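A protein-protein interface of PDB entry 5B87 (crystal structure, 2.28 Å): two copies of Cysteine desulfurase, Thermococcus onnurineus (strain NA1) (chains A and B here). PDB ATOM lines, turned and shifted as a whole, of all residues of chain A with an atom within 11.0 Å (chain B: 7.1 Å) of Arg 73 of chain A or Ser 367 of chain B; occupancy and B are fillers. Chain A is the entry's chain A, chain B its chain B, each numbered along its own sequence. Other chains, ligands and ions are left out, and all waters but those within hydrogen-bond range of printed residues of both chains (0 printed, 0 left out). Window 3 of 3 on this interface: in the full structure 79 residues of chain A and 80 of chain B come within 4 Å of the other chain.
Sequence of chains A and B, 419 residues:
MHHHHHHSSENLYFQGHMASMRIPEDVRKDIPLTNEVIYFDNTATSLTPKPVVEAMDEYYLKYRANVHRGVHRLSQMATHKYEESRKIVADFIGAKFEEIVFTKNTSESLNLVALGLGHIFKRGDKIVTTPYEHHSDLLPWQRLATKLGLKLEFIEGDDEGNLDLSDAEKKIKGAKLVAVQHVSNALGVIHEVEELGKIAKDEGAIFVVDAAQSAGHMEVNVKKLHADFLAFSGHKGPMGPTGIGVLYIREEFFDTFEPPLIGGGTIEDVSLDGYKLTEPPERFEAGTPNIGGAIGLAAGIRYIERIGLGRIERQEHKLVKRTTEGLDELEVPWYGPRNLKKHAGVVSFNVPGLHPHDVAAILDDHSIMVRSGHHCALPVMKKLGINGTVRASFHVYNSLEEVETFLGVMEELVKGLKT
No position is printed for both chains.
Of the 9 pairs that touch across the chains among the printed residues, none has its exchanged pair printed and touching as well.
Printed residues of chain B within 4 Å of Val 71 of chain A: Ala 361 (3.96 Å).
Printed residues of chain B within 4 Å of His 72 of chain A: Asp 364 and Met 369.
Of chain B, only Asp 364, Ser 367 and Met 369 come within 4 Å of Arg 73 of chain A.
Of the printed residues of chain B, Leu 74 of chain A touches Val 37 (3.9 Å), Tyr 39 (3.9 Å) and Met 369 (3.9 Å).
Val 37 of chain B touches just one residue of chain A: Leu 74 (3.9 Å).
No residue of chain A comes within 4 Å of Ile 38 of chain B.
Printed residues of chain A within 4 Å of Tyr 39 of chain B: Leu 74 (3.9 Å).
Printed residues of chain A within 4 Å of Ala 361 of chain B: Val 71 (3.96 Å).
Of chain A, only His 72 (3.3 Å) and Arg 73 (2.8 Å) come within 4 Å of Asp 364 of chain B.
Of chain A, only Arg 73 (2.4 Å) comes within 4 Å of Ser 367 of chain B.
The nearest residue of chain A that does not touch Ser 367 of chain B is His 72 of chain A (7.4 Å).
ND1 of His 72 of chain A lies close to N of Leu 74 of chain A (3.5 Å).
ND1 of His 72 of chain A lies within hydrogen-bond range of N of Ser 75 of chain A, 3.3 Å away.
N of Ile 38 of chain B is in hydrogen-bond range of O of Ser 367 of chain B.
O of Ile 38 of chain B sits at hydrogen-bond distance from N of Met 369 of chain B (3.0 Å).
Ala 361 of chain B touches Val 71 of chain A.
CA of His 72 of chain A touches OD1 of Asp 364 of chain B, at 3.3 Å.
Arg 73 of chain A touches Met 369 of chain B.
CD2 of Leu 74 of chain A touches CG2 of Val 37 of chain B, 3.9 Å away.
Tyr 39 of chain B touches Leu 74 of chain A (CD1 to CD2, 3.9 Å).
Leu 74 of chain A touches Met 369 of chain B (CD2 to CG, 3.9 Å).
Hydrophobic or aromatic side chains of chain A that line the printed part of chain B: Val 71, His 72 and Leu 74.
Hydrophobic or aromatic side chains of chain B that line the printed part of chain A: Val 37, Tyr 39, Ala 361 and Met 369.
Among the printed residues, 9 pairs touch across the chains.
Among the printed residues, Asp or Glu carboxylates within 4 Å of a Lys or Arg side-chain nitrogen of the other chain: Arg 73 of chain A with Asp 364 of chain B (3.7 Å).
The side-chain sulfur (SD) of Met 369 of chain B sits at hydrogen-bond distance from a ring nitrogen (ND1) of His 72 of chain A, 3.5 Å away.
The guanidinium group of Arg 73 of chain A is in salt-bridge range of the side-chain carboxylate of Asp 364 of chain B, at 3.7 Å.
NH2 of Arg 73 of chain A is in hydrogen-bond range of OG of Ser 367 of chain B.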
ATOM      1  N   TYR A  59     -18.027  10.193   2.972  1.00  0.00           N
ATOM      2  CA  TYR A  59     -17.512   9.115   2.188  1.00  0.00           C
ATOM      3  C   TYR A  59     -16.115   9.458   1.684  1.00  0.00           C
ATOM      4  O   TYR A  59     -15.232   8.700   1.875  1.00  0.00           O
ATOM      5  CB  TYR A  59     -18.405   8.771   0.991  1.00  0.00           C
ATOM      6  CG  TYR A  59     -17.747   7.913  -0.067  1.00  0.00           C
ATOM      7  CD1 TYR A  59     -17.467   6.585   0.169  1.00  0.00           C
ATOM      8  CD2 TYR A  59     -17.386   8.434  -1.293  1.00  0.00           C
ATOM      9  CE1 TYR A  59     -16.868   5.796  -0.772  1.00  0.00           C
ATOM     10  CE2 TYR A  59     -16.802   7.642  -2.255  1.00  0.00           C
ATOM     11  CZ  TYR A  59     -16.532   6.317  -1.984  1.00  0.00           C
ATOM     12  OH  TYR A  59     -15.942   5.513  -2.899  1.00  0.00           O
ATOM     13  N   LYS A  62     -13.664  10.045   5.124  1.00  0.00           N
ATOM     14  CA  LYS A  62     -13.654   9.086   6.238  1.00  0.00           C
ATOM     15  C   LYS A  62     -13.843   7.616   5.854  1.00  0.00           C
ATOM     16  O   LYS A  62     -13.419   6.745   6.644  1.00  0.00           O
ATOM     17  CB  LYS A  62     -14.759   9.419   7.246  1.00  0.00           C
ATOM     18  CG  LYS A  62     -14.532  10.647   8.127  1.00  0.00           C
ATOM     19  CD  LYS A  62     -15.864  11.217   8.590  1.00  0.00           C
ATOM     20  CE  LYS A  62     -15.795  11.859   9.981  1.00  0.00           C
ATOM     21  NZ  LYS A  62     -14.701  12.859  10.076  1.00  0.00           N
ATOM     22  N   TYR A  63     -14.514   7.289   4.725  1.00  0.00           N
ATOM     23  CA  TYR A  63     -14.627   5.856   4.374  1.00  0.00           C
ATOM     24  C   TYR A  63     -14.440   5.574   2.891  1.00  0.00           C
ATOM     25  O   TYR A  63     -15.104   4.727   2.294  1.00  0.00           O
ATOM     26  CB  TYR A  63     -15.881   5.175   4.991  1.00  0.00           C
ATOM     27  CG  TYR A  63     -17.225   5.742   4.583  1.00  0.00           C
ATOM     28  CD1 TYR A  63     -17.773   6.838   5.243  1.00  0.00           C
ATOM     29  CD2 TYR A  63     -17.958   5.166   3.546  1.00  0.00           C
ATOM     30  CE1 TYR A  63     -19.002   7.351   4.860  1.00  0.00           C
ATOM     31  CE2 TYR A  63     -19.208   5.674   3.159  1.00  0.00           C
ATOM     32  CZ  TYR A  63     -19.728   6.772   3.812  1.00  0.00           C
ATOM     33  OH  TYR A  63     -21.004   7.254   3.434  1.00  0.00           O
ATOM     34  N   ARG A  64     -13.502   6.281   2.313  1.00  0.00           N
ATOM     35  CA  ARG A  64     -13.205   6.194   0.926  1.00  0.00           C
ATOM     36  C   ARG A  64     -12.679   4.873   0.501  1.00  0.00           C
ATOM     37  O   ARG A  64     -11.644   4.475   0.910  1.00  0.00           O
ATOM     38  CB  ARG A  64     -12.230   7.282   0.558  1.00  0.00           C
ATOM     39  CG  ARG A  64     -11.932   7.361  -0.898  1.00  0.00           C
ATOM     40  CD  ARG A  64     -13.088   7.808  -1.752  1.00  0.00           C
ATOM     41  NE  ARG A  64     -12.502   8.091  -3.027  1.00  0.00           N
ATOM     42  CZ  ARG A  64     -12.556   7.311  -4.070  1.00  0.00           C
ATOM     43  NH1 ARG A  64     -11.915   7.615  -5.136  1.00  0.00           N
ATOM     44  NH2 ARG A  64     -13.254   6.236  -4.039  1.00  0.00           N
ATOM     45  N   ALA A  65     -13.416   4.211  -0.356  1.00  0.00           N
ATOM     46  CA  ALA A  65     -13.047   2.899  -0.851  1.00  0.00           C
ATOM     47  C   ALA A  65     -14.001   2.413  -1.920  1.00  0.00           C
ATOM     48  O   ALA A  65     -15.077   2.893  -2.025  1.00  0.00           O
ATOM     49  CB  ALA A  65     -13.028   1.905   0.293  1.00  0.00           C
ATOM     50  N   ASN A  66     -13.566   1.455  -2.698  1.00  0.00           N
ATOM     51  CA  ASN A  66     -14.381   0.874  -3.709  1.00  0.00           C
ATOM     52  C   ASN A  66     -15.332  -0.121  -3.065  1.00  0.00           C
ATOM     53  O   ASN A  66     -15.180  -0.468  -1.942  1.00  0.00           O
ATOM     54  CB  ASN A  66     -13.547   0.208  -4.780  1.00  0.00           C
ATOM     55  CG  ASN A  66     -14.250   0.167  -6.092  1.00  0.00           C
ATOM     56  OD1 ASN A  66     -15.435   0.045  -6.130  1.00  0.00           O
ATOM     57  ND2 ASN A  66     -13.524   0.287  -7.161  1.00  0.00           N
ATOM     58  N   VAL A  67     -16.314  -0.554  -3.813  1.00  0.00           N
ATOM     59  CA  VAL A  67     -17.323  -1.460  -3.322  1.00  0.00           C
ATOM     60  C   VAL A  67     -17.058  -2.915  -3.702  1.00  0.00           C
ATOM     61  O   VAL A  67     -16.021  -3.425  -3.433  1.00  0.00           O
ATOM     62  CB  VAL A  67     -18.717  -0.926  -3.689  1.00  0.00           C
ATOM     63  CG1 VAL A  67     -19.800  -1.877  -3.293  1.00  0.00           C
ATOM     64  CG2 VAL A  67     -18.978   0.316  -2.894  1.00  0.00           C
ATOM     65  N   HIS A  68     -17.997  -3.615  -4.319  1.00  0.00           N
ATOM     66  CA  HIS A  68     -17.814  -5.016  -4.689  1.00  0.00           C
ATOM     67  C   HIS A  68     -17.505  -5.680  -3.371  1.00  0.00           C
ATOM     68  O   HIS A  68     -18.178  -5.381  -2.397  1.00  0.00           O
ATOM     69  CB  HIS A  68     -16.655  -5.167  -5.686  1.00  0.00           C
ATOM     70  CG  HIS A  68     -16.587  -4.080  -6.731  1.00  0.00           C
ATOM     71  ND1 HIS A  68     -17.674  -3.694  -7.490  1.00  0.00           N
ATOM     72  CD2 HIS A  68     -15.549  -3.324  -7.162  1.00  0.00           C
ATOM     73  CE1 HIS A  68     -17.313  -2.739  -8.325  1.00  0.00           C
ATOM     74  NE2 HIS A  68     -16.029  -2.495  -8.149  1.00  0.00           N
ATOM     75  N   ARG A  69     -16.477  -6.506  -3.317  1.00  0.00           N
ATOM     76  CA  ARG A  69     -16.117  -7.035  -2.019  1.00  0.00           C
ATOM     77  C   ARG A  69     -14.698  -7.252  -1.628  1.00  0.00           C
ATOM     78  O   ARG A  69     -13.936  -8.005  -2.230  1.00  0.00           O
ATOM     79  CB  ARG A  69     -16.996  -8.161  -1.485  1.00  0.00           C
ATOM     80  CG  ARG A  69     -16.789  -8.272   0.025  1.00  0.00           C
ATOM     81  CD  ARG A  69     -17.307  -9.564   0.675  1.00  0.00           C
ATOM     82  NE  ARG A  69     -16.922  -9.625   2.084  1.00  0.00           N
ATOM     83  CZ  ARG A  69     -17.729  -9.917   3.098  1.00  0.00           C
ATOM     84  NH1 ARG A  69     -18.998 -10.226   2.897  1.00  0.00           N
ATOM     85  NH2 ARG A  69     -17.244  -9.921   4.324  1.00  0.00           N
ATOM     86  N   GLY A  70     -14.378  -6.552  -0.568  1.00  0.00           N
ATOM     87  CA  GLY A  70     -13.082  -6.719   0.080  1.00  0.00           C
ATOM     88  C   GLY A  70     -13.366  -6.987   1.541  1.00  0.00           C
ATOM     89  O   GLY A  70     -14.420  -6.611   2.042  1.00  0.00           O
ATOM     90  N   VAL A  71     -12.434  -7.615   2.247  1.00  0.00           N
ATOM     91  CA  VAL A  71     -12.588  -7.782   3.711  1.00  0.00           C
ATOM     92  C   VAL A  71     -12.307  -6.473   4.438  1.00  0.00           C
ATOM     93  O   VAL A  71     -12.896  -6.216   5.491  1.00  0.00           O
ATOM     94  CB  VAL A  71     -11.663  -8.857   4.343  1.00  0.00           C
ATOM     95  CG1 VAL A  71     -12.242  -9.300   5.711  1.00  0.00           C
ATOM     96  CG2 VAL A  71     -11.438 -10.041   3.391  1.00  0.00           C
ATOM     97  N   HIS A  72     -11.360  -5.700   3.944  1.00  0.00           N
ATOM     98  CA  HIS A  72     -10.963  -4.477   4.619  1.00  0.00           C
ATOM     99  C   HIS A  72     -12.081  -3.532   5.043  1.00  0.00           C
ATOM    100  O   HIS A  72     -13.060  -3.374   4.378  1.00  0.00           O
ATOM    101  CB  HIS A  72      -9.701  -3.850   4.028  1.00  0.00           C
ATOM    102  CG  HIS A  72      -9.919  -2.985   2.842  1.00  0.00           C
ATOM    103  ND1 HIS A  72     -10.593  -1.799   2.903  1.00  0.00           N
ATOM    104  CD2 HIS A  72      -9.493  -3.104   1.570  1.00  0.00           C
ATOM    105  CE1 HIS A  72     -10.604  -1.243   1.715  1.00  0.00           C
ATOM    106  NE2 HIS A  72      -9.950  -2.019   0.885  1.00  0.00           N
ATOM    107  N   ARG A  73     -11.917  -2.945   6.206  1.00  0.00           N
ATOM    108  CA  ARG A  73     -12.941  -2.132   6.772  1.00  0.00           C
ATOM    109  C   ARG A  73     -13.481  -0.981   5.956  1.00  0.00           C
ATOM    110  O   ARG A  73     -14.643  -0.750   5.971  1.00  0.00           O
ATOM    111  CB  ARG A  73     -12.586  -1.722   8.180  1.00  0.00           C
ATOM    112  CG  ARG A  73     -11.360  -0.874   8.325  1.00  0.00           C
ATOM    113  CD  ARG A  73     -11.300  -0.384   9.739  1.00  0.00           C
ATOM    114  NE  ARG A  73      -9.963  -0.316  10.265  1.00  0.00           N
ATOM    115  CZ  ARG A  73      -9.348  -1.313  10.871  1.00  0.00           C
ATOM    116  NH1 ARG A  73      -9.942  -2.467  11.030  1.00  0.00           N
ATOM    117  NH2 ARG A  73      -8.136  -1.138  11.318  1.00  0.00           N
ATOM    118  N   LEU A  74     -12.635  -0.260   5.261  1.00  0.00           N
ATOM    119  CA  LEU A  74     -13.094   0.855   4.411  1.00  0.00           C
ATOM    120  C   LEU A  74     -14.081   0.334   3.354  1.00  0.00           C
ATOM    121  O   LEU A  74     -15.131   0.913   3.167  1.00  0.00           O
ATOM    122  CB  LEU A  74     -11.921   1.621   3.790  1.00  0.00           C
ATOM    123  CG  LEU A  74     -11.363   2.855   4.511  1.00  0.00           C
ATOM    124  CD1 LEU A  74     -11.767   3.046   5.975  1.00  0.00           C
ATOM    125  CD2 LEU A  74      -9.860   2.905   4.326  1.00  0.00           C
ATOM    126  N   SER A  75     -13.795  -0.828   2.780  1.00  0.00           N
ATOM    127  CA  SER A  75     -14.598  -1.390   1.730  1.00  0.00           C
ATOM    128  C   SER A  75     -15.866  -1.936   2.284  1.00  0.00           C
ATOM    129  O   SER A  75     -16.897  -1.895   1.591  1.00  0.00           O
ATOM    130  CB  SER A  75     -13.841  -2.500   1.033  1.00  0.00           C
ATOM    131  OG  SER A  75     -14.553  -2.873  -0.122  1.00  0.00           O
ATOM    132  N   GLN A  76     -15.816  -2.438   3.520  1.00  0.00           N
ATOM    133  CA  GLN A  76     -17.052  -2.913   4.188  1.00  0.00           C
ATOM    134  C   GLN A  76     -18.020  -1.753   4.392  1.00  0.00           C
ATOM    135  O   GLN A  76     -19.226  -1.857   4.093  1.00  0.00           O
ATOM    136  CB  GLN A  76     -16.783  -3.609   5.540  1.00  0.00           C
ATOM    137  CG  GLN A  76     -16.066  -4.973   5.452  1.00  0.00           C
ATOM    138  CD  GLN A  76     -16.901  -6.036   4.736  1.00  0.00           C
ATOM    139  OE1 GLN A  76     -17.953  -6.442   5.226  1.00  0.00           O
ATOM    140  NE2 GLN A  76     -16.438  -6.497   3.575  1.00  0.00           N
ATOM    141  N   MET A  77     -17.505  -0.650   4.881  1.00  0.00           N
ATOM    142  CA  MET A  77     -18.308   0.515   5.089  1.00  0.00           C
ATOM    143  C   MET A  77     -18.877   1.113   3.788  1.00  0.00           C
ATOM    144  O   MET A  77     -20.022   1.415   3.716  1.00  0.00           O
ATOM    145  CB  MET A  77     -17.515   1.523   5.893  1.00  0.00           C
ATOM    146  CG  MET A  77     -18.300   2.684   6.437  1.00  0.00           C
ATOM    147  SD  MET A  77     -19.810   2.263   7.298  1.00  0.00           S
ATOM    148  CE  MET A  77     -19.307   2.683   8.941  1.00  0.00           C
ATOM    149  N   ALA A  78     -18.049   1.245   2.777  1.00  0.00           N
ATOM    150  CA  ALA A  78     -18.462   1.774   1.504  1.00  0.00           C
ATOM    151  C   ALA A  78     -19.546   0.911   0.908  1.00  0.00           C
ATOM    152  O   ALA A  78     -20.523   1.402   0.458  1.00  0.00           O
ATOM    153  CB  ALA A  78     -17.293   1.904   0.563  1.00  0.00           C
ATOM    154  N   THR A  79     -19.339  -0.386   0.933  1.00  0.00           N
ATOM    155  CA  THR A  79     -20.292  -1.355   0.446  1.00  0.00           C
ATOM    156  C   THR A  79     -21.620  -1.209   1.187  1.00  0.00           C
ATOM    157  O   THR A  79     -22.652  -1.074   0.581  1.00  0.00           O
ATOM    158  CB  THR A  79     -19.728  -2.767   0.572  1.00  0.00           C
ATOM    159  OG1 THR A  79     -18.404  -2.771   0.066  1.00  0.00           O
ATOM    160  CG2 THR A  79     -20.524  -3.716  -0.220  1.00  0.00           C
ATOM    161  N   HIS A  80     -21.567  -1.221   2.504  1.00  0.00           N
ATOM    162  CA  HIS A  80     -22.762  -0.995   3.337  1.00  0.00           C
ATOM    163  C   HIS A  80     -23.527   0.288   3.012  1.00  0.00           C
ATOM    164  O   HIS A  80     -24.778   0.251   2.966  1.00  0.00           O
ATOM    165  CB  HIS A  80     -22.399  -0.994   4.845  1.00  0.00           C
ATOM    166  CG  HIS A  80     -23.539  -0.641   5.761  1.00  0.00           C
ATOM    167  ND1 HIS A  80     -24.549  -1.528   6.082  1.00  0.00           N
ATOM    168  CD2 HIS A  80     -23.801   0.489   6.467  1.00  0.00           C
ATOM    169  CE1 HIS A  80     -25.396  -0.949   6.918  1.00  0.00           C
ATOM    170  NE2 HIS A  80     -24.971   0.279   7.158  1.00  0.00           N
ATOM    171  N   LYS A  81     -22.810   1.416   2.878  1.00  0.00           N
ATOM    172  CA  LYS A  81     -23.473   2.709   2.518  1.00  0.00           C
ATOM    173  C   LYS A  81     -24.018   2.757   1.094  1.00  0.00           C
ATOM    174  O   LYS A  81     -25.039   3.375   0.873  1.00  0.00           O
ATOM    175  CB  LYS A  81     -22.554   3.899   2.701  1.00  0.00           C
ATOM    176  CG  LYS A  81     -22.170   4.096   4.151  1.00  0.00           C
ATOM    177  CD  LYS A  81     -23.289   4.511   5.080  1.00  0.00           C
ATOM    178  CE  LYS A  81     -23.856   5.861   4.750  1.00  0.00           C
ATOM    179  NZ  LYS A  81     -24.976   6.221   5.651  1.00  0.00           N
ATOM    180  N   TYR A  82     -23.350   2.094   0.174  1.00  0.00           N
ATOM    181  CA  TYR A  82     -23.782   2.003  -1.182  1.00  0.00           C
ATOM    182  C   TYR A  82     -25.058   1.181  -1.263  1.00  0.00           C
ATOM    183  O   TYR A  82     -25.965   1.536  -1.943  1.00  0.00           O
ATOM    184  CB  TYR A  82     -22.711   1.370  -2.024  1.00  0.00           C
ATOM    185  CG  TYR A  82     -23.047   1.308  -3.467  1.00  0.00           C
ATOM    186  CD1 TYR A  82     -23.284   2.444  -4.191  1.00  0.00           C
ATOM    187  CD2 TYR A  82     -23.142   0.101  -4.110  1.00  0.00           C
ATOM    188  CE1 TYR A  82     -23.591   2.380  -5.518  1.00  0.00           C
ATOM    189  CE2 TYR A  82     -23.440   0.032  -5.432  1.00  0.00           C
ATOM    190  CZ  TYR A  82     -23.672   1.177  -6.126  1.00  0.00           C
ATOM    191  OH  TYR A  82     -23.989   1.094  -7.422  1.00  0.00           O
ATOM    192  N   GLU B  36      -5.181   7.174   9.770  1.00  0.00           N
ATOM    193  CA  GLU B  36      -5.958   6.101  10.337  1.00  0.00           C
ATOM    194  C   GLU B  36      -5.586   4.707   9.890  1.00  0.00           C
ATOM    195  O   GLU B  36      -5.595   3.815  10.684  1.00  0.00           O
ATOM    196  CB  GLU B  36      -7.444   6.307  10.066  1.00  0.00           C
ATOM    197  CG  GLU B  36      -8.015   7.643  10.462  1.00  0.00           C
ATOM    198  CD  GLU B  36      -8.071   7.850  11.954  1.00  0.00           C
ATOM    199  OE1 GLU B  36      -7.313   8.687  12.468  1.00  0.00           O
ATOM    200  OE2 GLU B  36      -8.878   7.179  12.617  1.00  0.00           O
ATOM    201  N   VAL B  37      -5.287   4.538   8.616  1.00  0.00           N
ATOM    202  CA  VAL B  37      -4.938   3.255   8.064  1.00  0.00           C
ATOM    203  C   VAL B  37      -3.739   3.326   7.159  1.00  0.00           C
ATOM    204  O   VAL B  37      -3.263   4.376   6.861  1.00  0.00           O
ATOM    205  CB  VAL B  37      -6.087   2.657   7.218  1.00  0.00           C
ATOM    206  CG1 VAL B  37      -7.286   2.346   8.046  1.00  0.00           C
ATOM    207  CG2 VAL B  37      -6.478   3.531   6.058  1.00  0.00           C
ATOM    208  N   ILE B  38      -3.282   2.172   6.726  1.00  0.00           N
ATOM    209  CA  ILE B  38      -2.215   2.036   5.772  1.00  0.00           C
ATOM    210  C   ILE B  38      -3.048   1.643   4.560  1.00  0.00           C
ATOM    211  O   ILE B  38      -3.574   0.565   4.517  1.00  0.00           O
ATOM    212  CB  ILE B  38      -1.200   0.995   6.220  1.00  0.00           C
ATOM    213  CG1 ILE B  38      -0.340   1.578   7.319  1.00  0.00           C
ATOM    214  CG2 ILE B  38      -0.293   0.596   5.092  1.00  0.00           C
ATOM    215  CD1 ILE B  38       0.776   0.683   7.775  1.00  0.00           C
ATOM    216  N   TYR B  39      -3.212   2.547   3.606  1.00  0.00           N
ATOM    217  CA  TYR B  39      -4.109   2.282   2.510  1.00  0.00           C
ATOM    218  C   TYR B  39      -3.278   1.740   1.339  1.00  0.00           C
ATOM    219  O   TYR B  39      -2.581   2.501   0.663  1.00  0.00           O
ATOM    220  CB  TYR B  39      -4.937   3.524   2.094  1.00  0.00           C
ATOM    221  CG  TYR B  39      -6.026   3.214   1.058  1.00  0.00           C
ATOM    222  CD1 TYR B  39      -7.261   2.666   1.420  1.00  0.00           C
ATOM    223  CD2 TYR B  39      -5.767   3.348  -0.283  1.00  0.00           C
ATOM    224  CE1 TYR B  39      -8.235   2.347   0.443  1.00  0.00           C
ATOM    225  CE2 TYR B  39      -6.712   3.035  -1.228  1.00  0.00           C
ATOM    226  CZ  TYR B  39      -7.947   2.529  -0.853  1.00  0.00           C
ATOM    227  OH  TYR B  39      -8.872   2.291  -1.844  1.00  0.00           O
ATOM    228  N   ALA B 361      -7.722 -10.317   5.609  1.00  0.00           N
ATOM    229  CA  ALA B 361      -8.408 -10.156   6.945  1.00  0.00           C
ATOM    230  C   ALA B 361      -7.439  -9.928   8.064  1.00  0.00           C
ATOM    231  O   ALA B 361      -7.664  -9.058   8.875  1.00  0.00           O
ATOM    232  CB  ALA B 361      -9.259 -11.375   7.293  1.00  0.00           C
ATOM    233  N   ILE B 362      -6.354 -10.702   8.140  1.00  0.00           N
ATOM    234  CA  ILE B 362      -5.332 -10.443   9.189  1.00  0.00           C
ATOM    235  C   ILE B 362      -4.694  -9.067   9.014  1.00  0.00           C
ATOM    236  O   ILE B 362      -4.442  -8.342   9.986  1.00  0.00           O
ATOM    237  CB  ILE B 362      -4.225 -11.541   9.230  1.00  0.00           C
ATOM    238  CG1 ILE B 362      -4.831 -12.838   9.816  1.00  0.00           C
ATOM    239  CG2 ILE B 362      -3.027 -11.097  10.074  1.00  0.00           C
ATOM    240  CD1 ILE B 362      -3.988 -14.077   9.606  1.00  0.00           C
ATOM    241  N   LEU B 363      -4.395  -8.733   7.772  1.00  0.00           N
ATOM    242  CA  LEU B 363      -3.831  -7.418   7.451  1.00  0.00           C
ATOM    243  C   LEU B 363      -4.839  -6.299   7.864  1.00  0.00           C
ATOM    244  O   LEU B 363      -4.475  -5.349   8.569  1.00  0.00           O
ATOM    245  CB  LEU B 363      -3.466  -7.361   5.966  1.00  0.00           C
ATOM    246  CG  LEU B 363      -2.087  -7.447   5.315  1.00  0.00           C
ATOM    247  CD1 LEU B 363      -0.894  -7.755   6.206  1.00  0.00           C
ATOM    248  CD2 LEU B 363      -2.114  -8.301   4.065  1.00  0.00           C
ATOM    249  N   ASP B 364      -6.101  -6.441   7.501  1.00  0.00           N
ATOM    250  CA  ASP B 364      -7.151  -5.508   8.022  1.00  0.00           C
ATOM    251  C   ASP B 364      -7.227  -5.366   9.595  1.00  0.00           C
ATOM    252  O   ASP B 364      -7.313  -4.235  10.138  1.00  0.00           O
ATOM    253  CB  ASP B 364      -8.522  -5.862   7.420  1.00  0.00           C
ATOM    254  CG  ASP B 364      -9.641  -4.963   7.931  1.00  0.00           C
ATOM    255  OD1 ASP B 364      -9.648  -3.760   7.610  1.00  0.00           O
ATOM    256  OD2 ASP B 364     -10.512  -5.455   8.659  1.00  0.00           O
ATOM    257  N   ASP B 365      -7.158  -6.468  10.352  1.00  0.00           N
ATOM    258  CA  ASP B 365      -7.067  -6.348  11.847  1.00  0.00           C
ATOM    259  C   ASP B 365      -5.855  -5.494  12.267  1.00  0.00           C
ATOM    260  O   ASP B 365      -5.872  -4.918  13.324  1.00  0.00           O
ATOM    261  CB  ASP B 365      -6.952  -7.707  12.597  1.00  0.00           C
ATOM    262  CG  ASP B 365      -8.084  -8.697  12.272  1.00  0.00           C
ATOM    263  OD1 ASP B 365      -9.291  -8.332  12.216  1.00  0.00           O
ATOM    264  OD2 ASP B 365      -7.742  -9.883  12.107  1.00  0.00           O
ATOM    265  N   HIS B 366      -4.805  -5.402  11.457  1.00  0.00           N
ATOM    266  CA  HIS B 366      -3.681  -4.477  11.779  1.00  0.00           C
ATOM    267  C   HIS B 366      -3.786  -3.146  11.025  1.00  0.00           C
ATOM    268  O   HIS B 366      -2.804  -2.430  10.870  1.00  0.00           O
ATOM    269  CB  HIS B 366      -2.335  -5.114  11.451  1.00  0.00           C
ATOM    270  CG  HIS B 366      -1.923  -6.202  12.386  1.00  0.00           C
ATOM    271  ND1 HIS B 366      -2.445  -7.478  12.323  1.00  0.00           N
ATOM    272  CD2 HIS B 366      -0.992  -6.223  13.367  1.00  0.00           C
ATOM    273  CE1 HIS B 366      -1.876  -8.230  13.247  1.00  0.00           C
ATOM    274  NE2 HIS B 366      -0.988  -7.495  13.889  1.00  0.00           N
ATOM    275  N   SER B 367      -4.973  -2.812  10.527  1.00  0.00           N
ATOM    276  CA  SER B 367      -5.196  -1.513   9.867  1.00  0.00           C
ATOM    277  C   SER B 367      -4.448  -1.340   8.561  1.00  0.00           C
ATOM    278  O   SER B 367      -4.103  -0.210   8.191  1.00  0.00           O
ATOM    279  CB  SER B 367      -4.913  -0.336  10.834  1.00  0.00           C
ATOM    280  OG  SER B 367      -5.910  -0.309  11.864  1.00  0.00           O
ATOM    281  N   ILE B 368      -4.186  -2.442   7.868  1.00  0.00           N
ATOM    282  CA  ILE B 368      -3.563  -2.387   6.557  1.00  0.00           C
ATOM    283  C   ILE B 368      -4.644  -2.881   5.569  1.00  0.00           C
ATOM    284  O   ILE B 368      -5.072  -4.030   5.673  1.00  0.00           O
ATOM    285  CB  ILE B 368      -2.318  -3.273   6.490  1.00  0.00           C
ATOM    286  CG1 ILE B 368      -1.166  -2.658   7.277  1.00  0.00           C
ATOM    287  CG2 ILE B 368      -1.873  -3.534   5.052  1.00  0.00           C
ATOM    288  CD1 ILE B 368      -0.147  -3.653   7.778  1.00  0.00           C
ATOM    289  N   MET B 369      -5.046  -1.997   4.633  1.00  0.00           N
ATOM    290  CA  MET B 369      -6.057  -2.270   3.638  1.00  0.00           C
ATOM    291  C   MET B 369      -5.454  -2.819   2.367  1.00  0.00           C
ATOM    292  O   MET B 369      -4.674  -2.162   1.655  1.00  0.00           O
ATOM    293  CB  MET B 369      -6.871  -0.992   3.269  1.00  0.00           C
ATOM    294  CG  MET B 369      -7.380  -0.121   4.420  1.00  0.00           C
ATOM    295  SD  MET B 369      -8.533  -0.831   5.582  1.00  0.00           S
ATOM    296  CE  MET B 369      -7.480  -1.505   6.847  1.00  0.00           C
